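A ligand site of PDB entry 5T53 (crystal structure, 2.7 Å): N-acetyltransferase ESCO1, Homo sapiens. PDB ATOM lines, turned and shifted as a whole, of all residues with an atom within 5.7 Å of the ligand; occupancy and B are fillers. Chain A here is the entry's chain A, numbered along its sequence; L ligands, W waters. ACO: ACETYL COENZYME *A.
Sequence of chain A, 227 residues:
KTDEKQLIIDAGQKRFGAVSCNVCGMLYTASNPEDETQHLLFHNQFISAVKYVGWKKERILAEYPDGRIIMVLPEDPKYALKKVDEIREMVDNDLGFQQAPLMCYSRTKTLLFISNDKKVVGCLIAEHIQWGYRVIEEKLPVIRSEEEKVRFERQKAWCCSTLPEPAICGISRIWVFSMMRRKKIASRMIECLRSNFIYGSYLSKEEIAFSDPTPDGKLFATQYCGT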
ATOM      1  N   LEU A  95       9.138  14.158  -9.132  1.00  0.00           N
ATOM      2  CA  LEU A  95       9.512  15.480  -8.636  1.00  0.00           C
ATOM      3  C   LEU A  95      10.969  15.579  -8.216  1.00  0.00           C
ATOM      4  O   LEU A  95      11.533  16.674  -8.239  1.00  0.00           O
ATOM      5  CB  LEU A  95       8.629  15.876  -7.439  1.00  0.00           C
ATOM      6  CG  LEU A  95       7.120  15.791  -7.657  1.00  0.00           C
ATOM      7  CD1 LEU A  95       6.347  15.990  -6.361  1.00  0.00           C
ATOM      8  CD2 LEU A  95       6.686  16.783  -8.717  1.00  0.00           C
ATOM      9  N   ILE A 171      -1.088  19.644   3.844  1.00  0.00           N
ATOM     10  CA  ILE A 171      -0.944  18.978   2.544  1.00  0.00           C
ATOM     11  C   ILE A 171       0.542  18.731   2.303  1.00  0.00           C
ATOM     12  O   ILE A 171       1.315  19.677   2.182  1.00  0.00           O
ATOM     13  CB  ILE A 171      -1.547  19.801   1.419  1.00  0.00           C
ATOM     14  CG1 ILE A 171      -3.066  19.970   1.586  1.00  0.00           C
ATOM     15  CG2 ILE A 171      -1.207  19.161   0.078  1.00  0.00           C
ATOM     16  CD1 ILE A 171      -3.645  21.036   0.643  1.00  0.00           C
ATOM     17  N   SER A 172       0.926  17.465   2.194  1.00  0.00           N
ATOM     18  CA  SER A 172       2.324  17.122   1.974  1.00  0.00           C
ATOM     19  C   SER A 172       2.657  16.925   0.494  1.00  0.00           C
ATOM     20  O   SER A 172       3.803  17.142   0.090  1.00  0.00           O
ATOM     21  CB  SER A 172       2.673  15.867   2.769  1.00  0.00           C
ATOM     22  OG  SER A 172       4.067  15.769   2.984  1.00  0.00           O
ATOM     23  N   ARG A 173       1.671  16.514  -0.310  1.00  0.00           N
ATOM     24  CA  ARG A 173       1.912  16.139  -1.692  1.00  0.00           C
ATOM     25  C   ARG A 173       0.634  16.358  -2.493  1.00  0.00           C
ATOM     26  O   ARG A 173      -0.447  15.942  -2.078  1.00  0.00           O
ATOM     27  CB  ARG A 173       2.382  14.670  -1.804  1.00  0.00           C
ATOM     28  N   ILE A 174       0.782  17.039  -3.638  1.00  0.00           N
ATOM     29  CA  ILE A 174      -0.323  17.299  -4.559  1.00  0.00           C
ATOM     30  C   ILE A 174       0.225  17.034  -5.966  1.00  0.00           C
ATOM     31  O   ILE A 174       1.147  17.721  -6.419  1.00  0.00           O
ATOM     32  CB  ILE A 174      -0.884  18.738  -4.419  1.00  0.00           C
ATOM     33  CG1 ILE A 174      -2.095  18.995  -5.320  1.00  0.00           C
ATOM     34  CG2 ILE A 174       0.159  19.827  -4.660  1.00  0.00           C
ATOM     35  CD1 ILE A 174      -3.351  18.343  -4.836  1.00  0.00           C
ATOM     36  N   TRP A 175      -0.281  16.010  -6.625  1.00  0.00           N
ATOM     37  CA  TRP A 175       0.289  15.619  -7.903  1.00  0.00           C
ATOM     38  C   TRP A 175      -0.806  15.143  -8.838  1.00  0.00           C
ATOM     39  O   TRP A 175      -1.708  14.401  -8.419  1.00  0.00           O
ATOM     40  CB  TRP A 175       1.342  14.505  -7.775  1.00  0.00           C
ATOM     41  CG  TRP A 175       1.657  13.813  -9.090  1.00  0.00           C
ATOM     42  CD1 TRP A 175       2.667  14.134  -9.959  1.00  0.00           C
ATOM     43  CD2 TRP A 175       0.936  12.729  -9.689  1.00  0.00           C
ATOM     44  NE1 TRP A 175       2.620  13.297 -11.055  1.00  0.00           N
ATOM     45  CE2 TRP A 175       1.575  12.429 -10.912  1.00  0.00           C
ATOM     46  CE3 TRP A 175      -0.173  11.972  -9.308  1.00  0.00           C
ATOM     47  CZ2 TRP A 175       1.135  11.409 -11.750  1.00  0.00           C
ATOM     48  CZ3 TRP A 175      -0.623  10.954 -10.147  1.00  0.00           C
ATOM     49  CH2 TRP A 175       0.035  10.693 -11.354  1.00  0.00           C
ATOM     50  N   VAL A 176      -0.719  15.579 -10.089  1.00  0.00           N
ATOM     51  CA  VAL A 176      -1.601  15.100 -11.135  1.00  0.00           C
ATOM     52  C   VAL A 176      -0.761  14.854 -12.384  1.00  0.00           C
ATOM     53  O   VAL A 176       0.165  15.609 -12.680  1.00  0.00           O
ATOM     54  CB  VAL A 176      -2.768  16.084 -11.387  1.00  0.00           C
ATOM     55  CG1 VAL A 176      -3.363  16.516 -10.061  1.00  0.00           C
ATOM     56  CG2 VAL A 176      -2.309  17.276 -12.162  1.00  0.00           C
ATOM     57  N   PHE A 177      -1.063  13.761 -13.092  1.00  0.00           N
ATOM     58  CA  PHE A 177      -0.222  13.308 -14.200  1.00  0.00           C
ATOM     59  C   PHE A 177      -0.217  14.349 -15.304  1.00  0.00           C
ATOM     60  O   PHE A 177      -1.259  14.864 -15.700  1.00  0.00           O
ATOM     61  CB  PHE A 177      -0.735  11.961 -14.707  1.00  0.00           C
ATOM     62  CG  PHE A 177      -0.129  11.497 -16.005  1.00  0.00           C
ATOM     63  CD1 PHE A 177       1.241  11.362 -16.140  1.00  0.00           C
ATOM     64  CD2 PHE A 177      -0.944  11.081 -17.052  1.00  0.00           C
ATOM     65  CE1 PHE A 177       1.798  10.900 -17.335  1.00  0.00           C
ATOM     66  CE2 PHE A 177      -0.411  10.609 -18.234  1.00  0.00           C
ATOM     67  CZ  PHE A 177       0.972  10.523 -18.375  1.00  0.00           C
ATOM     68  N   MET A 180      -2.672  15.060 -17.936  1.00  0.00           N
ATOM     69  CA  MET A 180      -4.023  15.334 -17.479  1.00  0.00           C
ATOM     70  C   MET A 180      -4.142  16.681 -16.795  1.00  0.00           C
ATOM     71  O   MET A 180      -5.231  17.022 -16.316  1.00  0.00           O
ATOM     72  CB  MET A 180      -4.496  14.227 -16.520  1.00  0.00           C
ATOM     73  CG  MET A 180      -4.426  12.801 -17.081  1.00  0.00           C
ATOM     74  SD  MET A 180      -5.732  12.404 -18.251  1.00  0.00           S
ATOM     75  CE  MET A 180      -7.178  12.516 -17.200  1.00  0.00           C
ATOM     76  N   ARG A 181      -3.061  17.461 -16.738  1.00  0.00           N
ATOM     77  CA  ARG A 181      -3.037  18.730 -16.015  1.00  0.00           C
ATOM     78  C   ARG A 181      -3.970  19.742 -16.674  1.00  0.00           C
ATOM     79  O   ARG A 181      -4.554  19.511 -17.736  1.00  0.00           O
ATOM     80  CB  ARG A 181      -1.604  19.265 -15.933  1.00  0.00           C
ATOM     81  CG  ARG A 181      -0.834  18.677 -14.764  1.00  0.00           C
ATOM     82  CD  ARG A 181       0.675  18.849 -14.808  1.00  0.00           C
ATOM     83  NE  ARG A 181       1.315  17.829 -13.973  1.00  0.00           N
ATOM     84  CZ  ARG A 181       2.622  17.624 -13.908  1.00  0.00           C
ATOM     85  NH1 ARG A 181       3.453  18.362 -14.630  1.00  0.00           N
ATOM     86  NH2 ARG A 181       3.101  16.651 -13.121  1.00  0.00           N
ATOM     87  N   ARG A 182      -4.127  20.888 -16.001  1.00  0.00           N
ATOM     88  CA  ARG A 182      -4.987  21.978 -16.427  1.00  0.00           C
ATOM     89  C   ARG A 182      -6.426  21.529 -16.700  1.00  0.00           C
ATOM     90  O   ARG A 182      -7.150  22.182 -17.453  1.00  0.00           O
ATOM     91  CB  ARG A 182      -4.433  22.688 -17.675  1.00  0.00           C
ATOM     92  CG  ARG A 182      -2.991  23.177 -17.579  1.00  0.00           C
ATOM     93  CD  ARG A 182      -2.764  24.071 -16.382  1.00  0.00           C
ATOM     94  NE  ARG A 182      -3.694  25.200 -16.309  1.00  0.00           N
ATOM     95  CZ  ARG A 182      -3.361  26.452 -16.583  1.00  0.00           C
ATOM     96  NH1 ARG A 182      -4.270  27.416 -16.496  1.00  0.00           N
ATOM     97  NH2 ARG A 182      -2.118  26.754 -16.916  1.00  0.00           N
ATOM     98  N   LYS A 183      -6.881  20.428 -16.108  1.00  0.00           N
ATOM     99  CA  LYS A 183      -8.245  19.937 -16.269  1.00  0.00           C
ATOM    100  C   LYS A 183      -9.029  20.007 -14.961  1.00  0.00           C
ATOM    101  O   LYS A 183      -9.940  19.214 -14.714  1.00  0.00           O
ATOM    102  CB  LYS A 183      -8.247  18.513 -16.822  1.00  0.00           C
ATOM    103  CG  LYS A 183      -7.600  18.368 -18.191  1.00  0.00           C
ATOM    104  N   LYS A 184      -8.654  20.977 -14.107  1.00  0.00           N
ATOM    105  CA  LYS A 184      -9.359  21.270 -12.854  1.00  0.00           C
ATOM    106  C   LYS A 184      -9.528  20.035 -11.971  1.00  0.00           C
ATOM    107  O   LYS A 184     -10.530  19.918 -11.242  1.00  0.00           O
ATOM    108  CB  LYS A 184     -10.713  21.943 -13.131  1.00  0.00           C
ATOM    109  N   ILE A 185      -8.562  19.120 -11.975  1.00  0.00           N
ATOM    110  CA  ILE A 185      -8.734  17.875 -11.220  1.00  0.00           C
ATOM    111  C   ILE A 185      -8.001  17.916  -9.879  1.00  0.00           C
ATOM    112  O   ILE A 185      -8.427  17.263  -8.925  1.00  0.00           O
ATOM    113  CB  ILE A 185      -8.330  16.631 -12.059  1.00  0.00           C
ATOM    114  CG1 ILE A 185      -6.823  16.474 -12.304  1.00  0.00           C
ATOM    115  CG2 ILE A 185      -9.085  16.587 -13.395  1.00  0.00           C
ATOM    116  CD1 ILE A 185      -6.127  15.453 -11.394  1.00  0.00           C
ATOM    117  N   ALA A 186      -6.926  18.695  -9.737  1.00  0.00           N
ATOM    118  CA  ALA A 186      -6.405  18.970  -8.403  1.00  0.00           C
ATOM    119  C   ALA A 186      -7.376  19.812  -7.613  1.00  0.00           C
ATOM    120  O   ALA A 186      -7.552  19.594  -6.401  1.00  0.00           O
ATOM    121  CB  ALA A 186      -5.049  19.702  -8.453  1.00  0.00           C
ATOM    122  N   SER A 187      -8.012  20.775  -8.270  1.00  0.00           N
ATOM    123  CA  SER A 187      -9.066  21.562  -7.650  1.00  0.00           C
ATOM    124  C   SER A 187     -10.160  20.665  -7.085  1.00  0.00           C
ATOM    125  O   SER A 187     -10.710  20.948  -6.012  1.00  0.00           O
ATOM    126  CB  SER A 187      -9.640  22.542  -8.665  1.00  0.00           C
ATOM    127  OG  SER A 187      -8.645  23.451  -9.103  1.00  0.00           O
ATOM    128  N   ARG A 188     -10.484  19.577  -7.766  1.00  0.00           N
ATOM    129  CA  ARG A 188     -11.464  18.632  -7.242  1.00  0.00           C
ATOM    130  C   ARG A 188     -10.908  17.784  -6.114  1.00  0.00           C
ATOM    131  O   ARG A 188     -11.684  17.256  -5.308  1.00  0.00           O
ATOM    132  CB  ARG A 188     -11.993  17.750  -8.363  1.00  0.00           C
ATOM    133  CG  ARG A 188     -13.219  18.310  -9.050  1.00  0.00           C
ATOM    134  CD  ARG A 188     -13.022  18.443 -10.544  1.00  0.00           C
ATOM    135  NE  ARG A 188     -13.063  17.156 -11.233  1.00  0.00           N
ATOM    136  CZ  ARG A 188     -12.536  16.948 -12.442  1.00  0.00           C
ATOM    137  NH1 ARG A 188     -12.626  15.756 -13.007  1.00  0.00           N
ATOM    138  NH2 ARG A 188     -11.929  17.941 -13.080  1.00  0.00           N
ATOM    139  N   PHE A 210       0.227  23.680   4.078  1.00  0.00           N
ATOM    140  CA  PHE A 210       0.873  22.767   3.141  1.00  0.00           C
ATOM    141  C   PHE A 210       2.385  22.912   3.247  1.00  0.00           C
ATOM    142  O   PHE A 210       2.897  23.886   3.800  1.00  0.00           O
ATOM    143  CB  PHE A 210       0.401  23.007   1.702  1.00  0.00           C
ATOM    144  CG  PHE A 210       0.450  24.441   1.259  1.00  0.00           C
ATOM    145  CD1 PHE A 210      -0.581  25.318   1.583  1.00  0.00           C
ATOM    146  CD2 PHE A 210       1.507  24.908   0.495  1.00  0.00           C
ATOM    147  CE1 PHE A 210      -0.547  26.653   1.166  1.00  0.00           C
ATOM    148  CE2 PHE A 210       1.541  26.243   0.078  1.00  0.00           C
ATOM    149  CZ  PHE A 210       0.518  27.110   0.410  1.00  0.00           C
ATOM    150  N   SER A 211       3.080  21.909   2.731  1.00  0.00           N
ATOM    151  CA  SER A 211       4.535  21.961   2.754  1.00  0.00           C
ATOM    152  C   SER A 211       5.025  22.872   1.631  1.00  0.00           C
ATOM    153  O   SER A 211       4.278  23.201   0.703  1.00  0.00           O
ATOM    154  CB  SER A 211       5.132  20.556   2.659  1.00  0.00           C
ATOM    155  OG  SER A 211       4.667  19.855   1.524  1.00  0.00           O
ATOM    156  N   ASP A 212       6.284  23.296   1.747  1.00  0.00           N
ATOM    157  CA  ASP A 212       6.775  24.381   0.902  1.00  0.00           C
ATOM    158  C   ASP A 212       6.686  23.985  -0.548  1.00  0.00           C
ATOM    159  O   ASP A 212       7.132  22.886  -0.935  1.00  0.00           O
ATOM    160  CB  ASP A 212       8.206  24.798   1.302  1.00  0.00           C
ATOM    161  CG  ASP A 212       9.127  23.611   1.576  1.00  0.00           C
ATOM    162  OD1 ASP A 212      10.264  23.630   1.055  1.00  0.00           O
ATOM    163  OD2 ASP A 212       8.732  22.673   2.309  1.00  0.00           O
ATOM    164  N   PRO A 213       6.097  24.812  -1.430  1.00  0.00           N
ATOM    165  CA  PRO A 213       5.594  24.335  -2.702  1.00  0.00           C
ATOM    166  C   PRO A 213       6.652  24.354  -3.803  1.00  0.00           C
ATOM    167  O   PRO A 213       7.755  24.872  -3.655  1.00  0.00           O
ATOM    168  CB  PRO A 213       4.464  25.320  -3.029  1.00  0.00           C
ATOM    169  CG  PRO A 213       4.360  26.249  -1.844  1.00  0.00           C
ATOM    170  CD  PRO A 213       5.691  26.204  -1.172  1.00  0.00           C
ATOM    171  N   THR A 214       6.267  23.772  -4.924  1.00  0.00           N
ATOM    172  CA  THR A 214       6.976  23.922  -6.179  1.00  0.00           C
ATOM    173  C   THR A 214       6.373  25.070  -6.960  1.00  0.00           C
ATOM    174  O   THR A 214       5.346  25.639  -6.567  1.00  0.00           O
ATOM    175  CB  THR A 214       6.878  22.622  -6.972  1.00  0.00           C
ATOM    176  OG1 THR A 214       5.509  22.218  -7.077  1.00  0.00           O
ATOM    177  CG2 THR A 214       7.713  21.539  -6.329  1.00  0.00           C
ATOM    178  N   ASP A 216       4.750  24.786  -9.707  1.00  0.00           N
ATOM    179  CA  ASP A 216       3.399  24.340 -10.037  1.00  0.00           C
ATOM    180  C   ASP A 216       2.475  24.483  -8.832  1.00  0.00           C
ATOM    181  O   ASP A 216       1.356  24.979  -8.950  1.00  0.00           O
ATOM    182  CB  ASP A 216       3.429  22.899 -10.524  1.00  0.00           C
ATOM    183  CG  ASP A 216       4.302  22.711 -11.748  1.00  0.00           C
ATOM    184  OD1 ASP A 216       5.311  23.440 -11.854  1.00  0.00           O
ATOM    185  OD2 ASP A 216       3.998  21.832 -12.575  1.00  0.00           O
ATOM    186  N   GLY A 217       2.950  24.045  -7.650  1.00  0.00           N
ATOM    187  CA  GLY A 217       2.169  24.226  -6.432  1.00  0.00           C
ATOM    188  C   GLY A 217       1.832  25.689  -6.182  1.00  0.00           C
ATOM    189  O   GLY A 217       0.691  26.024  -5.843  1.00  0.00           O
ATOM    190  N   LEU A 219       1.794  28.064  -8.603  1.00  0.00           N
ATOM    191  CA  LEU A 219       0.864  28.447  -9.665  1.00  0.00           C
ATOM    192  C   LEU A 219      -0.537  27.888  -9.425  1.00  0.00           C
ATOM    193  O   LEU A 219      -1.516  28.476  -9.886  1.00  0.00           O
ATOM    194  CB  LEU A 219       1.402  27.979 -11.032  1.00  0.00           C
ATOM    195  N   PHE A 220      -0.644  26.773  -8.707  1.00  0.00           N
ATOM    196  CA  PHE A 220      -1.948  26.224  -8.353  1.00  0.00           C
ATOM    197  C   PHE A 220      -2.547  26.907  -7.124  1.00  0.00           C
ATOM    198  O   PHE A 220      -3.765  26.879  -6.929  1.00  0.00           O
ATOM    199  CB  PHE A 220      -1.845  24.716  -8.111  1.00  0.00           C
ATOM    200  CG  PHE A 220      -3.109  24.093  -7.571  1.00  0.00           C
ATOM    201  CD1 PHE A 220      -4.275  24.109  -8.322  1.00  0.00           C
ATOM    202  CD2 PHE A 220      -3.122  23.487  -6.336  1.00  0.00           C
ATOM    203  CE1 PHE A 220      -5.429  23.542  -7.836  1.00  0.00           C
ATOM    204  CE2 PHE A 220      -4.290  22.908  -5.837  1.00  0.00           C
ATOM    205  CZ  PHE A 220      -5.441  22.943  -6.594  1.00  0.00           C
ATOM    206  N   ALA A 221      -1.709  27.526  -6.286  1.00  0.00           N
ATOM    207  CA  ALA A 221      -2.206  28.082  -5.036  1.00  0.00           C
ATOM    208  C   ALA A 221      -2.874  29.441  -5.245  1.00  0.00           C
ATOM    209  O   ALA A 221      -3.957  29.698  -4.704  1.00  0.00           O
ATOM    210  CB  ALA A 221      -1.076  28.176  -4.010  1.00  0.00           C
ATOM    211  N   THR A 222      -2.244  30.309  -6.032  1.00  0.00           N
ATOM    212  CA  THR A 222      -2.813  31.630  -6.291  1.00  0.00           C
ATOM    213  C   THR A 222      -4.194  31.563  -6.932  1.00  0.00           C
ATOM    214  O   THR A 222      -4.895  32.576  -6.977  1.00  0.00           O
ATOM    215  CB  THR A 222      -1.862  32.432  -7.173  1.00  0.00           C
ATOM    216  OG1 THR A 222      -1.704  31.790  -8.444  1.00  0.00           O
ATOM    217  CG2 THR A 222      -0.505  32.546  -6.477  1.00  0.00           C
ATOM    218  N   GLN A 223      -4.580  30.397  -7.448  1.00  0.00           N
ATOM    219  CA  GLN A 223      -5.996  30.108  -7.640  1.00  0.00           C
ATOM    220  C   GLN A 223      -6.799  30.505  -6.415  1.00  0.00           C
ATOM    221  O   GLN A 223      -7.800  31.235  -6.536  1.00  0.00           O
ATOM    222  CB  GLN A 223      -6.174  28.602  -7.910  1.00  0.00           C
ATOM    223  CG  GLN A 223      -7.611  28.133  -7.722  1.00  0.00           C
ATOM    224  CD  GLN A 223      -8.026  27.082  -8.715  1.00  0.00           C
ATOM    225  OE1 GLN A 223      -7.396  26.888  -9.745  1.00  0.00           O
ATOM    226  NE2 GLN A 223      -9.065  26.346  -8.378  1.00  0.00           N
HETATM  227  N1A ACO L   1      -0.072  25.218 -13.833  1.00  0.00           N
HETATM  228  C2A ACO L   1      -1.068  24.858 -13.000  1.00  0.00           C
HETATM  229  N3A ACO L   1      -1.986  25.699 -12.631  1.00  0.00           N
HETATM  230  C4A ACO L   1      -1.974  26.981 -13.065  1.00  0.00           C
HETATM  231  C5A ACO L   1      -0.950  27.408 -13.924  1.00  0.00           C
HETATM  232  C6A ACO L   1       0.024  26.452 -14.303  1.00  0.00           C
HETATM  233  N6A ACO L   1       1.035  26.794 -15.122  1.00  0.00           N
HETATM  234  N7A ACO L   1      -1.189  28.731 -14.192  1.00  0.00           N
HETATM  235  C8A ACO L   1      -2.314  29.105 -13.532  1.00  0.00           C
HETATM  236  N9A ACO L   1      -2.799  28.081 -12.842  1.00  0.00           N
HETATM  237  C1B ACO L   1      -3.922  28.117 -12.072  1.00  0.00           C
HETATM  238  C2B ACO L   1      -5.105  28.309 -12.999  1.00  0.00           C
HETATM  239  O2B ACO L   1      -6.016  29.195 -12.452  1.00  0.00           O
HETATM  240  C3B ACO L   1      -5.687  26.968 -13.115  1.00  0.00           C
HETATM  241  O3B ACO L   1      -7.077  27.074 -13.350  1.00  0.00           O
HETATM  242  P3B ACO L   1      -7.597  27.182 -14.851  1.00  0.00           P
HETATM  243  O7A ACO L   1      -7.178  28.517 -15.451  1.00  0.00           O
HETATM  244  O8A ACO L   1      -7.022  26.057 -15.675  1.00  0.00           O
HETATM  245  O9A ACO L   1      -9.113  27.057 -14.850  1.00  0.00           O
HETATM  246  C4B ACO L   1      -5.392  26.380 -11.806  1.00  0.00           C
HETATM  247  O4B ACO L   1      -4.122  26.865 -11.376  1.00  0.00           O
HETATM  248  C5B ACO L   1      -5.239  24.855 -11.873  1.00  0.00           C
HETATM  249  O5B ACO L   1      -6.353  24.147 -11.399  1.00  0.00           O
HETATM  250  P1A ACO L   1      -6.245  22.550 -11.640  1.00  0.00           P
HETATM  251  O1A ACO L   1      -6.523  22.221 -13.098  1.00  0.00           O
HETATM  252  O2A ACO L   1      -7.239  21.788 -10.747  1.00  0.00           O
HETATM  253  O3A ACO L   1      -4.735  22.152 -11.327  1.00  0.00           O
HETATM  254  P2A ACO L   1      -3.939  20.949 -12.042  1.00  0.00           P
HETATM  255  O4A ACO L   1      -4.958  19.978 -12.564  1.00  0.00           O
HETATM  256  O5A ACO L   1      -3.092  21.442 -13.212  1.00  0.00           O
HETATM  257  O6A ACO L   1      -2.983  20.297 -10.952  1.00  0.00           O
HETATM  258  CBP ACO L   1      -0.875  20.657  -9.854  1.00  0.00           C
HETATM  259  CCP ACO L   1      -2.308  21.188 -10.082  1.00  0.00           C
HETATM  260  CDP ACO L   1      -0.936  19.594  -8.763  1.00  0.00           C
HETATM  261  CEP ACO L   1       0.048  21.762  -9.403  1.00  0.00           C
HETATM  262  CAP ACO L   1      -0.371  20.102 -11.189  1.00  0.00           C
HETATM  263  OAP ACO L   1       0.053  21.173 -12.011  1.00  0.00           O
HETATM  264  C9P ACO L   1       0.812  19.167 -10.999  1.00  0.00           C
HETATM  265  O9P ACO L   1       0.630  17.961 -10.791  1.00  0.00           O
HETATM  266  N8P ACO L   1       2.192  19.727 -11.084  1.00  0.00           N
HETATM  267  C7P ACO L   1       3.328  18.847 -10.911  1.00  0.00           C
HETATM  268  C6P ACO L   1       3.387  18.335  -9.514  1.00  0.00           C
HETATM  269  C5P ACO L   1       3.533  19.448  -8.442  1.00  0.00           C
HETATM  270  O5P ACO L   1       4.319  20.342  -8.628  1.00  0.00           O
HETATM  271  N4P ACO L   1       2.758  19.439  -7.241  1.00  0.00           N
HETATM  272  C3P ACO L   1       2.982  20.531  -6.312  1.00  0.00           C
HETATM  273  C2P ACO L   1       3.760  19.984  -5.128  1.00  0.00           C
HETATM  274  S1P ACO L   1       3.999  21.231  -3.906  1.00  0.00           S
HETATM  275  C   ACO L   1       3.796  20.376  -2.327  1.00  0.00           C
HETATM  276  O   ACO L   1       2.983  20.816  -1.500  1.00  0.00           O
HETATM  277  CH3 ACO L   1       4.102  18.880  -2.403  1.00  0.00           C
HETATM  278  O   HOH W   1       5.995  19.199  -7.032  1.00  0.00           O
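The side-chain hydroxyl (OG) of Ser 187 is in hydrogen-bond range of an oxygen (O2A) of the ligand.
The side-chain amide oxygen (OE1) of Gln 223 lies close to an oxygen (O5B) of the ligand, 3.4 Å away.
The backbone NH of Ile 185 is in hydrogen-bond range of an oxygen (O2A) of the ligand, 3.2 Å away.
O9P of the ligand is in hydrogen-bond range of N of Val 176 (2.8 Å).
The backbone NH (N) of Arg 182 is in hydrogen-bond range of an oxygen (O5A) of the ligand (3.0 Å).
An oxygen (O8A) of the ligand lies within salt-bridge range of the guanidinium group (NH1) of Arg 182 (3.2 Å).
An oxygen (O1A) of the ligand sits at hydrogen-bond distance from the backbone NH (N) of Lys 184 (2.7 Å).
OD2 of Asp 216 is in hydrogen-bond range of N8P of the ligand (3.1 Å).
The side-chain hydroxyl (OG1) of Thr 214 is in hydrogen-bond range of an oxygen (O5P) of the ligand (2.7 Å).
The backbone NH (N) of Ser 187 lies within hydrogen-bond range of an oxygen (O2A) of the ligand, 2.8 Å away.
S1P of the ligand lies close to N of Thr 214 (3.6 Å).
The backbone NH (N) of Ala 186 lies within hydrogen-bond range of an oxygen (O2A) of the ligand (3.3 Å).
An oxygen (O9P) of the ligand sits at hydrogen-bond distance from the guanidinium group of Arg 181, at 3.3 Å.
A nitrogen (N4P) of the ligand lies within hydrogen-bond range of the backbone carbonyl oxygen of Ile 174 (2.5 Å).
The backbone NH (N) of Ser 211 lies within hydrogen-bond range of the backbone carbonyl oxygen (O) of Ile 171, at 2.9 Å.
The backbone carbonyl oxygen (O) of Lys 184 sits close to the guanidinium group (NH2) of Arg 188 (3.0 Å).
O of Lys 183 is in hydrogen-bond range of NH2 of Arg 188, 2.9 Å away.
The backbone carbonyl oxygen (O) of Val 176 is in hydrogen-bond range of the guanidinium group (NE) of Arg 181.
The backbone NH of Gly 217 is in hydrogen-bond range of the side-chain hydroxyl of Thr 214, 3.2 Å away.
The side-chain amide nitrogen (NE2) of Gln 223 is in hydrogen-bond range of the side-chain hydroxyl (OG) of Ser 187.
The backbone carbonyl oxygen (O) of Ser 172 is in hydrogen-bond range of the side-chain hydroxyl (OG) of Ser 211 (3.2 Å).
The backbone carbonyl oxygen (O) of Ser 211 sits close to an oxygen (O) of the ligand, 3.5 Å away.
A nitrogen (N9A) of the ligand lies close to the backbone carbonyl oxygen (O) of Leu 219 (3.2 Å).
CD2 of Leu 95 touches C6P of the ligand, at 3.7 Å.
Ser 172 touches the ligand.
Arg 173 touches the ligand.
C of Trp 175 touches O9P of the ligand, at 3.7 Å.
Lys 183 touches the ligand (N to O1A, 3.5 Å).
Pro 213 touches the ligand.
Gly 217 touches the ligand (N to C3P, 3.8 Å).
CD1 of Phe 220 touches O3A of the ligand (3.6 Å).
Hydrophobic or aromatic side chains that line the ligand: Leu 95, Ile 174, Val 176, Ile 185, Ala 186, Leu 219 and Phe 220.
Within 4 Å of the ligand: Leu 95, Ser 172, Arg 173, Ile 174, Trp 175, Val 176, Arg 181, Arg 182, Lys 183, Lys 184, Ile 185, Ala 186, Ser 187, Ser 211, Pro 213, Thr 214, Asp 216, Gly 217, Leu 219, Phe 220 and Gln 223.
Water W1 lies within hydrogen-bond range of an oxygen (O5P) of the ligand and the side-chain hydroxyl (OG1) of Thr 214.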
